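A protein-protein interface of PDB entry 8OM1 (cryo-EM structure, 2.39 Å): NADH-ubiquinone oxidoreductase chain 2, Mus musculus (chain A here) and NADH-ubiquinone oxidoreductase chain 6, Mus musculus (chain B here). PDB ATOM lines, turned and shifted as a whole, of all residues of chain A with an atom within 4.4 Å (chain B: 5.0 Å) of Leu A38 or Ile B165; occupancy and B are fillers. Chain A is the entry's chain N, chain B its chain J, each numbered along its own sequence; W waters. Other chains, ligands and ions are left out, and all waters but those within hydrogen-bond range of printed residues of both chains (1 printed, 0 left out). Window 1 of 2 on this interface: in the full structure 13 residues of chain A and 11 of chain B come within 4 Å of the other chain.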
ATOM      1  N   GLU A  34      12.929  35.180  24.001  1.00  0.00           N
ATOM      2  CA  GLU A  34      12.485  34.342  22.893  1.00  0.00           C
ATOM      3  C   GLU A  34      13.645  33.585  22.267  1.00  0.00           C
ATOM      4  O   GLU A  34      13.498  32.414  21.911  1.00  0.00           O
ATOM      5  CB  GLU A  34      11.781  35.183  21.823  1.00  0.00           C
ATOM      6  CG  GLU A  34      10.428  35.782  22.200  1.00  0.00           C
ATOM      7  CD  GLU A  34       9.600  34.886  23.082  1.00  0.00           C
ATOM      8  OE1 GLU A  34       9.507  35.170  24.289  1.00  0.00           O
ATOM      9  OE2 GLU A  34       9.059  33.882  22.582  1.00  0.00           O
ATOM     10  N   PHE A  35      14.803  34.236  22.110  1.00  0.00           N
ATOM     11  CA  PHE A  35      15.957  33.544  21.547  1.00  0.00           C
ATOM     12  C   PHE A  35      16.358  32.365  22.419  1.00  0.00           C
ATOM     13  O   PHE A  35      16.718  31.301  21.909  1.00  0.00           O
ATOM     14  CB  PHE A  35      17.145  34.497  21.387  1.00  0.00           C
ATOM     15  CG  PHE A  35      17.130  35.303  20.116  1.00  0.00           C
ATOM     16  CD1 PHE A  35      16.930  34.703  18.886  1.00  0.00           C
ATOM     17  CD2 PHE A  35      17.331  36.663  20.153  1.00  0.00           C
ATOM     18  CE1 PHE A  35      16.922  35.452  17.734  1.00  0.00           C
ATOM     19  CE2 PHE A  35      17.324  37.411  19.000  1.00  0.00           C
ATOM     20  CZ  PHE A  35      17.117  36.804  17.793  1.00  0.00           C
ATOM     21  N   SER A  36      16.313  32.548  23.737  1.00  0.00           N
ATOM     22  CA  SER A  36      16.703  31.489  24.660  1.00  0.00           C
ATOM     23  C   SER A  36      15.811  30.267  24.509  1.00  0.00           C
ATOM     24  O   SER A  36      16.302  29.138  24.417  1.00  0.00           O
ATOM     25  CB  SER A  36      16.656  32.009  26.093  1.00  0.00           C
ATOM     26  OG  SER A  36      17.503  33.124  26.244  1.00  0.00           O
ATOM     27  N   LEU A  37      14.495  30.473  24.483  1.00  0.00           N
ATOM     28  CA  LEU A  37      13.581  29.346  24.353  1.00  0.00           C
ATOM     29  C   LEU A  37      13.824  28.599  23.049  1.00  0.00           C
ATOM     30  O   LEU A  37      14.005  27.379  23.045  1.00  0.00           O
ATOM     31  CB  LEU A  37      12.134  29.832  24.439  1.00  0.00           C
ATOM     32  CG  LEU A  37      11.041  28.840  24.016  1.00  0.00           C
ATOM     33  CD1 LEU A  37      11.137  27.551  24.816  1.00  0.00           C
ATOM     34  CD2 LEU A  37       9.676  29.447  24.170  1.00  0.00           C
ATOM     35  N   LEU A  38      13.859  29.325  21.933  1.00  0.00           N
ATOM     36  CA  LEU A  38      13.974  28.682  20.630  1.00  0.00           C
ATOM     37  C   LEU A  38      15.286  27.924  20.491  1.00  0.00           C
ATOM     38  O   LEU A  38      15.311  26.808  19.968  1.00  0.00           O
ATOM     39  CB  LEU A  38      13.847  29.728  19.526  1.00  0.00           C
ATOM     40  CG  LEU A  38      12.510  30.471  19.480  1.00  0.00           C
ATOM     41  CD1 LEU A  38      12.615  31.734  18.646  1.00  0.00           C
ATOM     42  CD2 LEU A  38      11.415  29.580  18.954  1.00  0.00           C
ATOM     43  N   ALA A  39      16.389  28.518  20.939  1.00  0.00           N
ATOM     44  CA  ALA A  39      17.698  27.924  20.701  1.00  0.00           C
ATOM     45  C   ALA A  39      17.954  26.716  21.596  1.00  0.00           C
ATOM     46  O   ALA A  39      18.681  25.801  21.200  1.00  0.00           O
ATOM     47  CB  ALA A  39      18.784  28.977  20.904  1.00  0.00           C
ATOM     48  N   ILE A  40      17.370  26.681  22.791  1.00  0.00           N
ATOM     49  CA  ILE A  40      17.661  25.592  23.716  1.00  0.00           C
ATOM     50  C   ILE A  40      16.878  24.322  23.397  1.00  0.00           C
ATOM     51  O   ILE A  40      17.316  23.234  23.773  1.00  0.00           O
ATOM     52  CB  ILE A  40      17.402  26.048  25.165  1.00  0.00           C
ATOM     53  CG1 ILE A  40      18.248  25.240  26.150  1.00  0.00           C
ATOM     54  CG2 ILE A  40      15.935  25.915  25.533  1.00  0.00           C
ATOM     55  CD1 ILE A  40      19.717  25.500  26.047  1.00  0.00           C
ATOM     56  N   ILE A  41      15.746  24.438  22.700  1.00  0.00           N
ATOM     57  CA  ILE A  41      14.927  23.262  22.405  1.00  0.00           C
ATOM     58  C   ILE A  41      15.693  22.204  21.619  1.00  0.00           C
ATOM     59  O   ILE A  41      15.632  21.023  21.996  1.00  0.00           O
ATOM     60  CB  ILE A  41      13.633  23.690  21.688  1.00  0.00           C
ATOM     61  CG1 ILE A  41      12.732  24.510  22.622  1.00  0.00           C
ATOM     62  CG2 ILE A  41      12.889  22.475  21.134  1.00  0.00           C
ATOM     63  CD1 ILE A  41      11.986  23.715  23.646  1.00  0.00           C
ATOM     64  N   PRO A  42      16.379  22.526  20.518  1.00  0.00           N
ATOM     65  CA  PRO A  42      17.099  21.467  19.796  1.00  0.00           C
ATOM     66  C   PRO A  42      18.170  20.791  20.628  1.00  0.00           C
ATOM     67  O   PRO A  42      18.442  19.603  20.426  1.00  0.00           O
ATOM     68  CB  PRO A  42      17.686  22.205  18.583  1.00  0.00           C
ATOM     69  CG  PRO A  42      17.660  23.625  18.947  1.00  0.00           C
ATOM     70  CD  PRO A  42      16.458  23.806  19.796  1.00  0.00           C
ATOM     71  N   ALA B 161      18.231  31.569  12.349  1.00  0.00           N
ATOM     72  CA  ALA B 161      18.496  30.513  13.311  1.00  0.00           C
ATOM     73  C   ALA B 161      17.356  29.507  13.355  1.00  0.00           C
ATOM     74  O   ALA B 161      17.589  28.321  13.599  1.00  0.00           O
ATOM     75  CB  ALA B 161      18.739  31.111  14.698  1.00  0.00           C
ATOM     76  N   GLY B 162      16.128  29.961  13.097  1.00  0.00           N
ATOM     77  CA  GLY B 162      14.996  29.055  13.071  1.00  0.00           C
ATOM     78  C   GLY B 162      15.142  27.942  12.054  1.00  0.00           C
ATOM     79  O   GLY B 162      14.698  26.820  12.292  1.00  0.00           O
ATOM     80  N   ILE B 163      15.768  28.228  10.914  1.00  0.00           N
ATOM     81  CA  ILE B 163      16.003  27.189   9.920  1.00  0.00           C
ATOM     82  C   ILE B 163      16.906  26.102  10.491  1.00  0.00           C
ATOM     83  O   ILE B 163      16.622  24.908  10.366  1.00  0.00           O
ATOM     84  CB  ILE B 163      16.600  27.797   8.639  1.00  0.00           C
ATOM     85  CG1 ILE B 163      15.569  28.685   7.942  1.00  0.00           C
ATOM     86  CG2 ILE B 163      17.077  26.699   7.714  1.00  0.00           C
ATOM     87  CD1 ILE B 163      16.170  29.638   6.951  1.00  0.00           C
ATOM     88  N   PHE B 164      18.002  26.501  11.137  1.00  0.00           N
ATOM     89  CA  PHE B 164      18.895  25.521  11.741  1.00  0.00           C
ATOM     90  C   PHE B 164      18.223  24.793  12.892  1.00  0.00           C
ATOM     91  O   PHE B 164      18.482  23.610  13.109  1.00  0.00           O
ATOM     92  CB  PHE B 164      20.181  26.196  12.219  1.00  0.00           C
ATOM     93  CG  PHE B 164      20.992  26.784  11.114  1.00  0.00           C
ATOM     94  CD1 PHE B 164      20.689  28.035  10.612  1.00  0.00           C
ATOM     95  CD2 PHE B 164      22.043  26.080  10.556  1.00  0.00           C
ATOM     96  CE1 PHE B 164      21.424  28.576   9.581  1.00  0.00           C
ATOM     97  CE2 PHE B 164      22.780  26.616   9.529  1.00  0.00           C
ATOM     98  CZ  PHE B 164      22.469  27.865   9.036  1.00  0.00           C
ATOM     99  N   ILE B 165      17.348  25.474  13.625  1.00  0.00           N
ATOM    100  CA  ILE B 165      16.675  24.843  14.754  1.00  0.00           C
ATOM    101  C   ILE B 165      15.708  23.766  14.277  1.00  0.00           C
ATOM    102  O   ILE B 165      15.721  22.639  14.780  1.00  0.00           O
ATOM    103  CB  ILE B 165      15.962  25.906  15.606  1.00  0.00           C
ATOM    104  CG1 ILE B 165      16.988  26.745  16.369  1.00  0.00           C
ATOM    105  CG2 ILE B 165      14.973  25.261  16.557  1.00  0.00           C
ATOM    106  CD1 ILE B 165      16.473  28.116  16.773  1.00  0.00           C
ATOM    107  N   ILE B 166      14.855  24.088  13.304  1.00  0.00           N
ATOM    108  CA  ILE B 166      13.822  23.131  12.917  1.00  0.00           C
ATOM    109  C   ILE B 166      14.433  21.946  12.185  1.00  0.00           C
ATOM    110  O   ILE B 166      13.900  20.837  12.243  1.00  0.00           O
ATOM    111  CB  ILE B 166      12.717  23.805  12.080  1.00  0.00           C
ATOM    112  CG1 ILE B 166      13.261  24.295  10.734  1.00  0.00           C
ATOM    113  CG2 ILE B 166      12.055  24.922  12.897  1.00  0.00           C
ATOM    114  CD1 ILE B 166      12.239  24.974   9.866  1.00  0.00           C
ATOM    115  N   ILE B 167      15.547  22.154  11.484  1.00  0.00           N
ATOM    116  CA  ILE B 167      16.234  21.031  10.857  1.00  0.00           C
ATOM    117  C   ILE B 167      16.782  20.083  11.919  1.00  0.00           C
ATOM    118  O   ILE B 167      16.733  18.860  11.758  1.00  0.00           O
ATOM    119  CB  ILE B 167      17.340  21.533   9.911  1.00  0.00           C
ATOM    120  CG1 ILE B 167      16.724  22.214   8.690  1.00  0.00           C
ATOM    121  CG2 ILE B 167      18.231  20.381   9.472  1.00  0.00           C
ATOM    122  CD1 ILE B 167      17.687  23.061   7.909  1.00  0.00           C
ATOM    123  N   GLU B 168      17.307  20.624  13.020  1.00  0.00           N
ATOM    124  CA  GLU B 168      17.809  19.762  14.085  1.00  0.00           C
ATOM    125  C   GLU B 168      16.686  19.040  14.810  1.00  0.00           C
ATOM    126  O   GLU B 168      16.812  17.853  15.119  1.00  0.00           O
ATOM    127  CB  GLU B 168      18.625  20.570  15.090  1.00  0.00           C
ATOM    128  CG  GLU B 168      20.011  20.929  14.648  1.00  0.00           C
ATOM    129  CD  GLU B 168      20.779  19.754  14.080  1.00  0.00           C
ATOM    130  OE1 GLU B 168      21.243  19.848  12.927  1.00  0.00           O
ATOM    131  OE2 GLU B 168      20.879  18.723  14.771  1.00  0.00           O
ATOM    132  N   ILE B 169      15.590  19.736  15.109  1.00  0.00           N
ATOM    133  CA  ILE B 169      14.499  19.099  15.837  1.00  0.00           C
ATOM    134  C   ILE B 169      13.941  17.927  15.040  1.00  0.00           C
ATOM    135  O   ILE B 169      13.580  16.891  15.607  1.00  0.00           O
ATOM    136  CB  ILE B 169      13.397  20.122  16.180  1.00  0.00           C
ATOM    137  CG1 ILE B 169      13.912  21.184  17.160  1.00  0.00           C
ATOM    138  CG2 ILE B 169      12.187  19.416  16.771  1.00  0.00           C
ATOM    139  CD1 ILE B 169      13.079  22.447  17.202  1.00  0.00           C
HETATM  140  O   HOH W   1      18.072  17.982  17.992  1.00  0.00           O
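Water W1 bridges the backbone carbonyl oxygen of Pro A42 (2.9 Å) and the backbone carbonyl oxygen of Glu B168 (3.1 Å).
Leu A38 touches just one residue of chain B: Ile B165 (3.6 Å). Of chain A, only Leu A38 (3.6 Å) and Pro A42 (3.8 Å) come within 4 Å of Ile B165. Printed residues of chain B within 4 Å of Pro A42: Ile B165 (3.8 Å) and Glu B168 (3.97 Å). Printed residues of chain B within 4 Å of Ile A41: Ile B169 (3.9 Å). Printed residues of chain A within 4 Å of Ile B169: Ile A41 (3.9 Å). Printed residues of chain A within 4 Å of Glu B168: Pro A42 (3.97 Å). Ile B166 touches none of the printed residues of chain A. Ile B163 touches none of the printed residues of chain A. The nearest printed residue of chain B that does not touch Leu A38 is Ile B169 (5.6 Å). The nearest residue of chain A that does not touch Ile B165 is Ala A39 (4.1 Å).
Hydrophobic or aromatic side chains of chain B within 4 Å of the printed part of chain A: Ile B165 and Ile B169. Hydrophobic or aromatic side chains of chain A that line the printed part of chain B: Ile A41 and Pro A42. Along chain A the printed residues that touch a printed residue of chain B span positions 38 to 42. Among the printed residues, 4 pairs touch across the chains. Among the printed residues, no Asp or Glu carboxylate lies within 4 Å of a Lys or Arg side-chain nitrogen of the other chain.
O of Leu A38 touches CD1 of Ile B165, at 3.6 Å. Ile B169 touches Ile A41 (CD1 to CG2, 3.9 Å). Ile B165 touches Pro A42 (CG2 to CD, 3.8 Å). Pro A42 touches Glu B168 (CB to CB, 3.97 Å).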
